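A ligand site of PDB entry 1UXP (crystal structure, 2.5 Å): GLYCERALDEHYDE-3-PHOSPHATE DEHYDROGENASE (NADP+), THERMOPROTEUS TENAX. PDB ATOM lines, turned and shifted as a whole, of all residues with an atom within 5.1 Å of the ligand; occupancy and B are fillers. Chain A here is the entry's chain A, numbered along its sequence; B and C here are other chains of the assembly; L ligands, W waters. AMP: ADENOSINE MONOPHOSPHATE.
NE1 of Trp 498 of chain C is in hydrogen-bond range of O2P of the ligand, at 3.0 Å.
An oxygen (O2') of the ligand lies within hydrogen-bond range of the side-chain carboxylate of Asp 141 of chain C (2.7 Å).
An oxygen (O3P) of the ligand lies within salt-bridge range of the guanidinium group (NH2) of Arg 72 (2.6 Å).
An oxygen (O3') of the ligand lies within hydrogen-bond range of the guanidinium group of Arg 79 (3.1 Å).
O2' of the ligand is in hydrogen-bond range of NE1 of Trp 142 of chain C.
O2P of the ligand lies within salt-bridge range of NH2 of Arg 154 (3.4 Å).
An oxygen (O1P) of the ligand is in salt-bridge range of the guanidinium group (NE) of Arg 440 of chain B.
A nitrogen (N6) of the ligand lies close to the backbone carbonyl oxygen of Gly 134 (3.2 Å).
The side-chain carboxylate of Asp 141 of chain C lies within hydrogen-bond range of the backbone NH of Gly 76 (3.0 Å).
The backbone NH (N) of Gly 135 lies within hydrogen-bond range of the backbone carbonyl oxygen (O) of Tyr 137 of chain C (3.3 Å).
The backbone carbonyl oxygen of Arg 440 of chain B lies within hydrogen-bond range of the guanidinium group of Arg 72, at 3.2 Å.
The backbone carbonyl oxygen (O) of Glu 156 sits close to the side-chain hydroxyl (OG1) of Thr 483 (3.5 Å).
The guanidinium group of Arg 79 sits at hydrogen-bond distance from the backbone carbonyl oxygen of Arg 72 (3.3 Å).
NH2 of Arg 72 is in salt-bridge range of OE2 of Glu 156, at 3.6 Å.
N of Gly 135 sits close to N6 of the ligand.
A nitrogen (N6) of the ligand sits close to the backbone NH (N) of Arg 155 (3.3 Å).
Residues that only touch the ligand: Tyr 137 of chain C, Ile 133, Pro 139 of chain C, Tyr 184, Glu 156, Lys 132 and Pro 157.
Hydrophobic or aromatic side chains within 4 Å of the ligand: Ile 133, Pro 157, Tyr 184, Tyr 137 of chain C, Pro 139 of chain C, Trp 142 of chain C and Trp 498 of chain C.
Within 4 Å of the ligand: Arg 72, Arg 79, Lys 132, Ile 133, Gly 134, Gly 135, Arg 154, Arg 155, Glu 156, Pro 157, Tyr 184, Arg 440 of chain B, Tyr 137 of chain C, Pro 139 of chain C, Asp 141 of chain C, Trp 142 of chain C and Trp 498 of chain C.
Water W1 lies within hydrogen-bond range of NH1 of Arg 154, OE2 of Glu 156, O3P of the ligand and O of Arg 155.
Water W3 lies within hydrogen-bond range of O1P of the ligand (2.8 Å), O of Arg 72 (2.9 Å) and O of Glu 501 of chain C (3.0 Å).
Water W4 lies within hydrogen-bond range of NH2 of Arg 436 of chain B (2.8 Å), O2P of the ligand (3.2 Å) and NH2 of Arg 154 (3.4 Å).
Water W2 lies within hydrogen-bond range of the side-chain carboxylate (OE2) of Glu 156 (2.4 Å), the guanidinium group (NH1) of Arg 154 (3.1 Å) and an oxygen (O3P) of the ligand (3.5 Å).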
ATOM      1  N   ARG A  72     -13.160  -9.379  13.725  1.00  0.00           N
ATOM      2  CA  ARG A  72     -12.852 -10.733  13.271  1.00  0.00           C
ATOM      3  C   ARG A  72     -13.725 -11.792  13.935  1.00  0.00           C
ATOM      4  O   ARG A  72     -14.126 -12.778  13.294  1.00  0.00           O
ATOM      5  CB  ARG A  72     -11.366 -11.041  13.535  1.00  0.00           C
ATOM      6  CG  ARG A  72     -10.861 -12.362  12.941  1.00  0.00           C
ATOM      7  CD  ARG A  72      -9.380 -12.595  13.229  1.00  0.00           C
ATOM      8  NE  ARG A  72      -8.932 -13.916  12.778  1.00  0.00           N
ATOM      9  CZ  ARG A  72      -7.706 -14.410  12.970  1.00  0.00           C
ATOM     10  NH1 ARG A  72      -6.778 -13.702  13.593  1.00  0.00           N
ATOM     11  NH2 ARG A  72      -7.422 -15.628  12.533  1.00  0.00           N
ATOM     12  N   GLY A  76     -19.071 -13.622   9.708  1.00  0.00           N
ATOM     13  CA  GLY A  76     -19.424 -12.942   8.470  1.00  0.00           C
ATOM     14  C   GLY A  76     -20.921 -12.721   8.298  1.00  0.00           C
ATOM     15  O   GLY A  76     -21.373 -11.660   7.839  1.00  0.00           O
ATOM     16  N   ARG A  79     -21.695  -9.682  10.049  1.00  0.00           N
ATOM     17  CA  ARG A  79     -21.094  -8.491   9.463  1.00  0.00           C
ATOM     18  C   ARG A  79     -21.981  -8.081   8.303  1.00  0.00           C
ATOM     19  O   ARG A  79     -22.200  -6.894   8.052  1.00  0.00           O
ATOM     20  CB  ARG A  79     -19.693  -8.771   8.917  1.00  0.00           C
ATOM     21  CG  ARG A  79     -18.725  -9.386   9.899  1.00  0.00           C
ATOM     22  CD  ARG A  79     -17.291  -9.092   9.483  1.00  0.00           C
ATOM     23  NE  ARG A  79     -16.379 -10.015  10.156  1.00  0.00           N
ATOM     24  CZ  ARG A  79     -15.789 -11.054   9.575  1.00  0.00           C
ATOM     25  NH1 ARG A  79     -15.990 -11.322   8.285  1.00  0.00           N
ATOM     26  NH2 ARG A  79     -15.022 -11.849  10.298  1.00  0.00           N
ATOM     27  N   LYS A 132     -14.900 -13.933  -4.041  1.00  0.00           N
ATOM     28  CA  LYS A 132     -13.447 -14.129  -4.012  1.00  0.00           C
ATOM     29  C   LYS A 132     -13.013 -14.653  -2.648  1.00  0.00           C
ATOM     30  O   LYS A 132     -11.869 -14.449  -2.213  1.00  0.00           O
ATOM     31  CB  LYS A 132     -12.709 -12.814  -4.312  1.00  0.00           C
ATOM     32  CG  LYS A 132     -12.934 -12.254  -5.697  1.00  0.00           C
ATOM     33  CD  LYS A 132     -12.564 -13.250  -6.802  1.00  0.00           C
ATOM     34  CE  LYS A 132     -12.829 -12.654  -8.192  1.00  0.00           C
ATOM     35  NZ  LYS A 132     -12.410 -13.537  -9.322  1.00  0.00           N
ATOM     36  N   ILE A 133     -13.937 -15.314  -1.956  1.00  0.00           N
ATOM     37  CA  ILE A 133     -13.639 -15.911  -0.668  1.00  0.00           C
ATOM     38  C   ILE A 133     -13.511 -17.411  -0.948  1.00  0.00           C
ATOM     39  O   ILE A 133     -14.321 -17.996  -1.686  1.00  0.00           O
ATOM     40  CB  ILE A 133     -14.758 -15.661   0.374  1.00  0.00           C
ATOM     41  CG1 ILE A 133     -14.464 -14.358   1.112  1.00  0.00           C
ATOM     42  CG2 ILE A 133     -14.847 -16.831   1.355  1.00  0.00           C
ATOM     43  CD1 ILE A 133     -15.307 -14.134   2.342  1.00  0.00           C
ATOM     44  N   GLY A 134     -12.500 -18.019  -0.352  1.00  0.00           N
ATOM     45  CA  GLY A 134     -12.272 -19.438  -0.555  1.00  0.00           C
ATOM     46  C   GLY A 134     -10.822 -19.637  -0.859  1.00  0.00           C
ATOM     47  O   GLY A 134     -10.228 -18.881  -1.616  1.00  0.00           O
ATOM     48  N   GLY A 135     -10.229 -20.666  -0.280  1.00  0.00           N
ATOM     49  CA  GLY A 135      -8.825 -20.895  -0.522  1.00  0.00           C
ATOM     50  C   GLY A 135      -8.513 -21.915  -1.582  1.00  0.00           C
ATOM     51  O   GLY A 135      -9.397 -22.400  -2.291  1.00  0.00           O
ATOM     52  N   VAL A 153      -4.236 -23.041   1.210  1.00  0.00           N
ATOM     53  CA  VAL A 153      -3.995 -21.603   1.184  1.00  0.00           C
ATOM     54  C   VAL A 153      -5.329 -20.840   1.358  1.00  0.00           C
ATOM     55  O   VAL A 153      -6.316 -21.093   0.681  1.00  0.00           O
ATOM     56  CB  VAL A 153      -3.345 -21.134  -0.141  1.00  0.00           C
ATOM     57  CG1 VAL A 153      -3.051 -19.616  -0.069  1.00  0.00           C
ATOM     58  CG2 VAL A 153      -2.069 -21.902  -0.390  1.00  0.00           C
ATOM     59  N   ARG A 154      -5.354 -19.902   2.283  1.00  0.00           N
ATOM     60  CA  ARG A 154      -6.573 -19.151   2.486  1.00  0.00           C
ATOM     61  C   ARG A 154      -6.244 -17.717   2.868  1.00  0.00           C
ATOM     62  O   ARG A 154      -5.067 -17.356   2.964  1.00  0.00           O
ATOM     63  CB  ARG A 154      -7.443 -19.828   3.539  1.00  0.00           C
ATOM     64  CG  ARG A 154      -6.694 -20.177   4.789  1.00  0.00           C
ATOM     65  CD  ARG A 154      -7.196 -19.350   5.914  1.00  0.00           C
ATOM     66  NE  ARG A 154      -8.343 -19.980   6.564  1.00  0.00           N
ATOM     67  CZ  ARG A 154      -9.248 -19.323   7.263  1.00  0.00           C
ATOM     68  NH1 ARG A 154      -9.159 -17.995   7.404  1.00  0.00           N
ATOM     69  NH2 ARG A 154     -10.225 -19.993   7.854  1.00  0.00           N
ATOM     70  N   ARG A 155      -7.274 -16.888   3.032  1.00  0.00           N
ATOM     71  CA  ARG A 155      -7.034 -15.495   3.383  1.00  0.00           C
ATOM     72  C   ARG A 155      -7.425 -15.205   4.810  1.00  0.00           C
ATOM     73  O   ARG A 155      -8.278 -15.880   5.408  1.00  0.00           O
ATOM     74  CB  ARG A 155      -7.748 -14.578   2.402  1.00  0.00           C
ATOM     75  CG  ARG A 155      -7.627 -15.118   0.986  1.00  0.00           C
ATOM     76  CD  ARG A 155      -7.993 -14.118  -0.088  1.00  0.00           C
ATOM     77  NE  ARG A 155      -6.837 -13.326  -0.487  1.00  0.00           N
ATOM     78  CZ  ARG A 155      -6.440 -13.175  -1.752  1.00  0.00           C
ATOM     79  NH1 ARG A 155      -7.132 -13.773  -2.737  1.00  0.00           N
ATOM     80  NH2 ARG A 155      -5.384 -12.403  -2.033  1.00  0.00           N
ATOM     81  N   GLU A 156      -6.767 -14.207   5.369  1.00  0.00           N
ATOM     82  CA  GLU A 156      -6.986 -13.826   6.744  1.00  0.00           C
ATOM     83  C   GLU A 156      -6.962 -12.298   6.783  1.00  0.00           C
ATOM     84  O   GLU A 156      -6.223 -11.682   6.031  1.00  0.00           O
ATOM     85  CB  GLU A 156      -5.854 -14.430   7.592  1.00  0.00           C
ATOM     86  CG  GLU A 156      -5.952 -14.228   9.082  1.00  0.00           C
ATOM     87  CD  GLU A 156      -5.158 -15.274   9.873  1.00  0.00           C
ATOM     88  OE1 GLU A 156      -4.266 -14.872  10.684  1.00  0.00           O
ATOM     89  OE2 GLU A 156      -5.457 -16.485   9.692  1.00  0.00           O
ATOM     90  N   PRO A 157      -7.815 -11.680   7.614  1.00  0.00           N
ATOM     91  CA  PRO A 157      -7.797 -10.213   7.677  1.00  0.00           C
ATOM     92  C   PRO A 157      -6.477  -9.735   8.279  1.00  0.00           C
ATOM     93  O   PRO A 157      -5.936 -10.354   9.204  1.00  0.00           O
ATOM     94  CB  PRO A 157      -9.005  -9.861   8.549  1.00  0.00           C
ATOM     95  CG  PRO A 157      -9.149 -11.062   9.439  1.00  0.00           C
ATOM     96  CD  PRO A 157      -8.890 -12.220   8.472  1.00  0.00           C
ATOM     97  N   TYR A 184     -14.350  -8.658   5.550  1.00  0.00           N
ATOM     98  CA  TYR A 184     -13.383  -9.740   5.722  1.00  0.00           C
ATOM     99  C   TYR A 184     -12.851  -9.906   7.153  1.00  0.00           C
ATOM    100  O   TYR A 184     -12.041 -10.797   7.427  1.00  0.00           O
ATOM    101  CB  TYR A 184     -12.222  -9.583   4.730  1.00  0.00           C
ATOM    102  CG  TYR A 184     -12.686  -9.621   3.278  1.00  0.00           C
ATOM    103  CD1 TYR A 184     -13.354 -10.728   2.786  1.00  0.00           C
ATOM    104  CD2 TYR A 184     -12.493  -8.531   2.429  1.00  0.00           C
ATOM    105  CE1 TYR A 184     -13.838 -10.754   1.489  1.00  0.00           C
ATOM    106  CE2 TYR A 184     -12.976  -8.535   1.121  1.00  0.00           C
ATOM    107  CZ  TYR A 184     -13.653  -9.649   0.651  1.00  0.00           C
ATOM    108  OH  TYR A 184     -14.150  -9.672  -0.642  1.00  0.00           O
ATOM    109  N   VAL A 479     -10.483  -7.540  -1.837  1.00  0.00           N
ATOM    110  CA  VAL A 479     -10.077  -8.476  -0.804  1.00  0.00           C
ATOM    111  C   VAL A 479      -8.534  -8.566  -0.740  1.00  0.00           C
ATOM    112  O   VAL A 479      -7.952  -8.676   0.335  1.00  0.00           O
ATOM    113  CB  VAL A 479     -10.655  -9.901  -1.069  1.00  0.00           C
ATOM    114  CG1 VAL A 479     -10.126 -10.450  -2.387  1.00  0.00           C
ATOM    115  CG2 VAL A 479     -10.315 -10.838   0.084  1.00  0.00           C
ATOM    116  N   THR A 483      -6.444  -8.137   3.116  1.00  0.00           N
ATOM    117  CA  THR A 483      -6.350  -9.507   3.507  1.00  0.00           C
ATOM    118  C   THR A 483      -4.955 -10.047   3.183  1.00  0.00           C
ATOM    119  O   THR A 483      -4.270  -9.546   2.287  1.00  0.00           O
ATOM    120  CB  THR A 483      -7.481 -10.230   2.751  1.00  0.00           C
ATOM    121  OG1 THR A 483      -8.518 -10.562   3.668  1.00  0.00           O
ATOM    122  CG2 THR A 483      -7.002 -11.424   2.002  1.00  0.00           C
ATOM    123  N   ARG B 436      -6.000 -27.130  14.546  1.00  0.00           N
ATOM    124  CA  ARG B 436      -6.821 -26.085  13.941  1.00  0.00           C
ATOM    125  C   ARG B 436      -6.743 -24.759  14.726  1.00  0.00           C
ATOM    126  O   ARG B 436      -6.644 -23.678  14.117  1.00  0.00           O
ATOM    127  CB  ARG B 436      -8.282 -26.544  13.820  1.00  0.00           C
ATOM    128  CG  ARG B 436      -9.104 -25.574  13.001  1.00  0.00           C
ATOM    129  CD  ARG B 436      -8.618 -25.547  11.546  1.00  0.00           C
ATOM    130  NE  ARG B 436      -9.232 -24.499  10.721  1.00  0.00           N
ATOM    131  CZ  ARG B 436      -8.946 -23.200  10.827  1.00  0.00           C
ATOM    132  NH1 ARG B 436      -8.085 -22.774  11.730  1.00  0.00           N
ATOM    133  NH2 ARG B 436      -9.482 -22.333   9.993  1.00  0.00           N
ATOM    134  N   ARG B 440      -5.224 -21.125  13.303  1.00  0.00           N
ATOM    135  CA  ARG B 440      -5.973 -19.895  13.260  1.00  0.00           C
ATOM    136  C   ARG B 440      -5.262 -18.760  13.987  1.00  0.00           C
ATOM    137  O   ARG B 440      -5.130 -17.647  13.451  1.00  0.00           O
ATOM    138  CB  ARG B 440      -7.365 -20.079  13.854  1.00  0.00           C
ATOM    139  CG  ARG B 440      -8.134 -18.766  13.962  1.00  0.00           C
ATOM    140  CD  ARG B 440      -9.579 -18.948  14.401  1.00  0.00           C
ATOM    141  NE  ARG B 440     -10.217 -17.641  14.430  1.00  0.00           N
ATOM    142  CZ  ARG B 440     -10.514 -16.955  15.532  1.00  0.00           C
ATOM    143  NH1 ARG B 440     -10.260 -17.449  16.737  1.00  0.00           N
ATOM    144  NH2 ARG B 440     -11.013 -15.723  15.415  1.00  0.00           N
ATOM    145  N   TYR C 137     -11.570 -24.111  -0.506  1.00  0.00           N
ATOM    146  CA  TYR C 137     -11.696 -24.094   0.937  1.00  0.00           C
ATOM    147  C   TYR C 137     -12.926 -23.239   1.194  1.00  0.00           C
ATOM    148  O   TYR C 137     -12.975 -22.091   0.752  1.00  0.00           O
ATOM    149  CB  TYR C 137     -10.489 -23.433   1.556  1.00  0.00           C
ATOM    150  CG  TYR C 137     -10.775 -22.961   2.942  1.00  0.00           C
ATOM    151  CD1 TYR C 137     -10.889 -23.886   3.995  1.00  0.00           C
ATOM    152  CD2 TYR C 137     -10.961 -21.594   3.211  1.00  0.00           C
ATOM    153  CE1 TYR C 137     -11.183 -23.453   5.299  1.00  0.00           C
ATOM    154  CE2 TYR C 137     -11.260 -21.149   4.512  1.00  0.00           C
ATOM    155  CZ  TYR C 137     -11.359 -22.079   5.547  1.00  0.00           C
ATOM    156  OH  TYR C 137     -11.617 -21.645   6.820  1.00  0.00           O
ATOM    157  N   PRO C 139     -15.032 -21.478   4.082  1.00  0.00           N
ATOM    158  CA  PRO C 139     -15.167 -21.169   5.527  1.00  0.00           C
ATOM    159  C   PRO C 139     -16.658 -21.245   5.898  1.00  0.00           C
ATOM    160  O   PRO C 139     -17.514 -21.020   5.035  1.00  0.00           O
ATOM    161  CB  PRO C 139     -14.602 -19.757   5.633  1.00  0.00           C
ATOM    162  CG  PRO C 139     -14.969 -19.169   4.306  1.00  0.00           C
ATOM    163  CD  PRO C 139     -14.691 -20.269   3.312  1.00  0.00           C
ATOM    164  N   ASP C 141     -18.489 -19.460   8.459  1.00  0.00           N
ATOM    165  CA  ASP C 141     -19.162 -18.396   9.204  1.00  0.00           C
ATOM    166  C   ASP C 141     -20.043 -17.486   8.385  1.00  0.00           C
ATOM    167  O   ASP C 141     -20.308 -16.352   8.803  1.00  0.00           O
ATOM    168  CB  ASP C 141     -18.135 -17.549   9.951  1.00  0.00           C
ATOM    169  CG  ASP C 141     -17.122 -16.936   9.020  1.00  0.00           C
ATOM    170  OD1 ASP C 141     -16.430 -17.703   8.310  1.00  0.00           O
ATOM    171  OD2 ASP C 141     -17.025 -15.684   8.993  1.00  0.00           O
ATOM    172  N   TRP C 142     -20.513 -17.959   7.228  1.00  0.00           N
ATOM    173  CA  TRP C 142     -21.362 -17.154   6.373  1.00  0.00           C
ATOM    174  C   TRP C 142     -22.805 -17.616   6.438  1.00  0.00           C
ATOM    175  O   TRP C 142     -23.653 -17.238   5.631  1.00  0.00           O
ATOM    176  CB  TRP C 142     -20.805 -17.163   4.929  1.00  0.00           C
ATOM    177  CG  TRP C 142     -19.503 -16.438   4.900  1.00  0.00           C
ATOM    178  CD1 TRP C 142     -18.245 -16.981   4.997  1.00  0.00           C
ATOM    179  CD2 TRP C 142     -19.320 -15.017   4.983  1.00  0.00           C
ATOM    180  NE1 TRP C 142     -17.300 -15.993   5.155  1.00  0.00           N
ATOM    181  CE2 TRP C 142     -17.922 -14.781   5.159  1.00  0.00           C
ATOM    182  CE3 TRP C 142     -20.197 -13.916   4.947  1.00  0.00           C
ATOM    183  CZ2 TRP C 142     -17.390 -13.489   5.293  1.00  0.00           C
ATOM    184  CZ3 TRP C 142     -19.661 -12.632   5.076  1.00  0.00           C
ATOM    185  CH2 TRP C 142     -18.280 -12.429   5.246  1.00  0.00           C
ATOM    186  N   TRP C 498     -12.888 -20.966  17.200  1.00  0.00           N
ATOM    187  CA  TRP C 498     -13.450 -19.636  17.013  1.00  0.00           C
ATOM    188  C   TRP C 498     -14.151 -19.188  18.303  1.00  0.00           C
ATOM    189  O   TRP C 498     -14.506 -20.037  19.144  1.00  0.00           O
ATOM    190  CB  TRP C 498     -14.463 -19.654  15.843  1.00  0.00           C
ATOM    191  CG  TRP C 498     -13.792 -19.800  14.505  1.00  0.00           C
ATOM    192  CD1 TRP C 498     -13.099 -18.828  13.825  1.00  0.00           C
ATOM    193  CD2 TRP C 498     -13.703 -20.987  13.711  1.00  0.00           C
ATOM    194  NE1 TRP C 498     -12.575 -19.350  12.669  1.00  0.00           N
ATOM    195  CE2 TRP C 498     -12.927 -20.672  12.563  1.00  0.00           C
ATOM    196  CE3 TRP C 498     -14.195 -22.297  13.855  1.00  0.00           C
ATOM    197  CZ2 TRP C 498     -12.633 -21.622  11.561  1.00  0.00           C
ATOM    198  CZ3 TRP C 498     -13.908 -23.232  12.864  1.00  0.00           C
ATOM    199  CH2 TRP C 498     -13.136 -22.891  11.734  1.00  0.00           C
ATOM    200  N   GLU C 501     -17.785 -17.063  15.741  1.00  0.00           N
ATOM    201  CA  GLU C 501     -17.384 -16.522  14.428  1.00  0.00           C
ATOM    202  C   GLU C 501     -16.853 -17.633  13.529  1.00  0.00           C
ATOM    203  O   GLU C 501     -15.986 -17.349  12.641  1.00  0.00           O
ATOM    204  CB  GLU C 501     -16.317 -15.464  14.581  1.00  0.00           C
ATOM    205  OXT GLU C 501     -17.334 -18.768  13.719  1.00  0.00           O
HETATM  206  P   AMP L   1     -10.654 -16.701  10.987  1.00  0.00           P
HETATM  207  O1P AMP L   1     -11.042 -16.365  12.370  1.00  0.00           O
HETATM  208  O2P AMP L   1     -11.116 -17.960  10.394  1.00  0.00           O
HETATM  209  O3P AMP L   1      -9.163 -16.523  10.810  1.00  0.00           O
HETATM  210  O5' AMP L   1     -11.361 -15.529  10.162  1.00  0.00           O
HETATM  211  C5' AMP L   1     -11.169 -15.485   8.778  1.00  0.00           C
HETATM  212  C4' AMP L   1     -12.287 -14.617   8.209  1.00  0.00           C
HETATM  213  O4' AMP L   1     -11.939 -14.612   6.793  1.00  0.00           O
HETATM  214  C3' AMP L   1     -13.774 -15.373   8.365  1.00  0.00           C
HETATM  215  O3' AMP L   1     -14.788 -14.262   8.435  1.00  0.00           O
HETATM  216  C2' AMP L   1     -13.756 -16.193   7.012  1.00  0.00           C
HETATM  217  O2' AMP L   1     -15.016 -16.434   6.447  1.00  0.00           O
HETATM  218  C1' AMP L   1     -12.907 -15.275   6.004  1.00  0.00           C
HETATM  219  N9  AMP L   1     -12.176 -16.069   5.007  1.00  0.00           N
HETATM  220  C8  AMP L   1     -11.805 -17.420   5.078  1.00  0.00           C
HETATM  221  N7  AMP L   1     -11.138 -17.932   4.017  1.00  0.00           N
HETATM  222  C5  AMP L   1     -11.107 -16.793   3.220  1.00  0.00           C
HETATM  223  C6  AMP L   1     -10.551 -16.594   1.916  1.00  0.00           C
HETATM  224  N6  AMP L   1      -9.952 -17.669   1.299  1.00  0.00           N
HETATM  225  N1  AMP L   1     -10.674 -15.302   1.388  1.00  0.00           N
HETATM  226  C2  AMP L   1     -11.286 -14.278   2.048  1.00  0.00           C
HETATM  227  N3  AMP L   1     -11.850 -14.378   3.284  1.00  0.00           N
HETATM  228  C4  AMP L   1     -11.717 -15.644   3.802  1.00  0.00           C
HETATM  229  O   HOH W   1      -7.792 -16.329   8.642  1.00  0.00           O
HETATM  230  O   HOH W   2      -6.757 -18.514   9.302  1.00  0.00           O
HETATM  231  O   HOH W   3     -13.723 -15.450  12.322  1.00  0.00           O
HETATM  232  O   HOH W   4      -8.613 -19.855  10.891  1.00  0.00           O
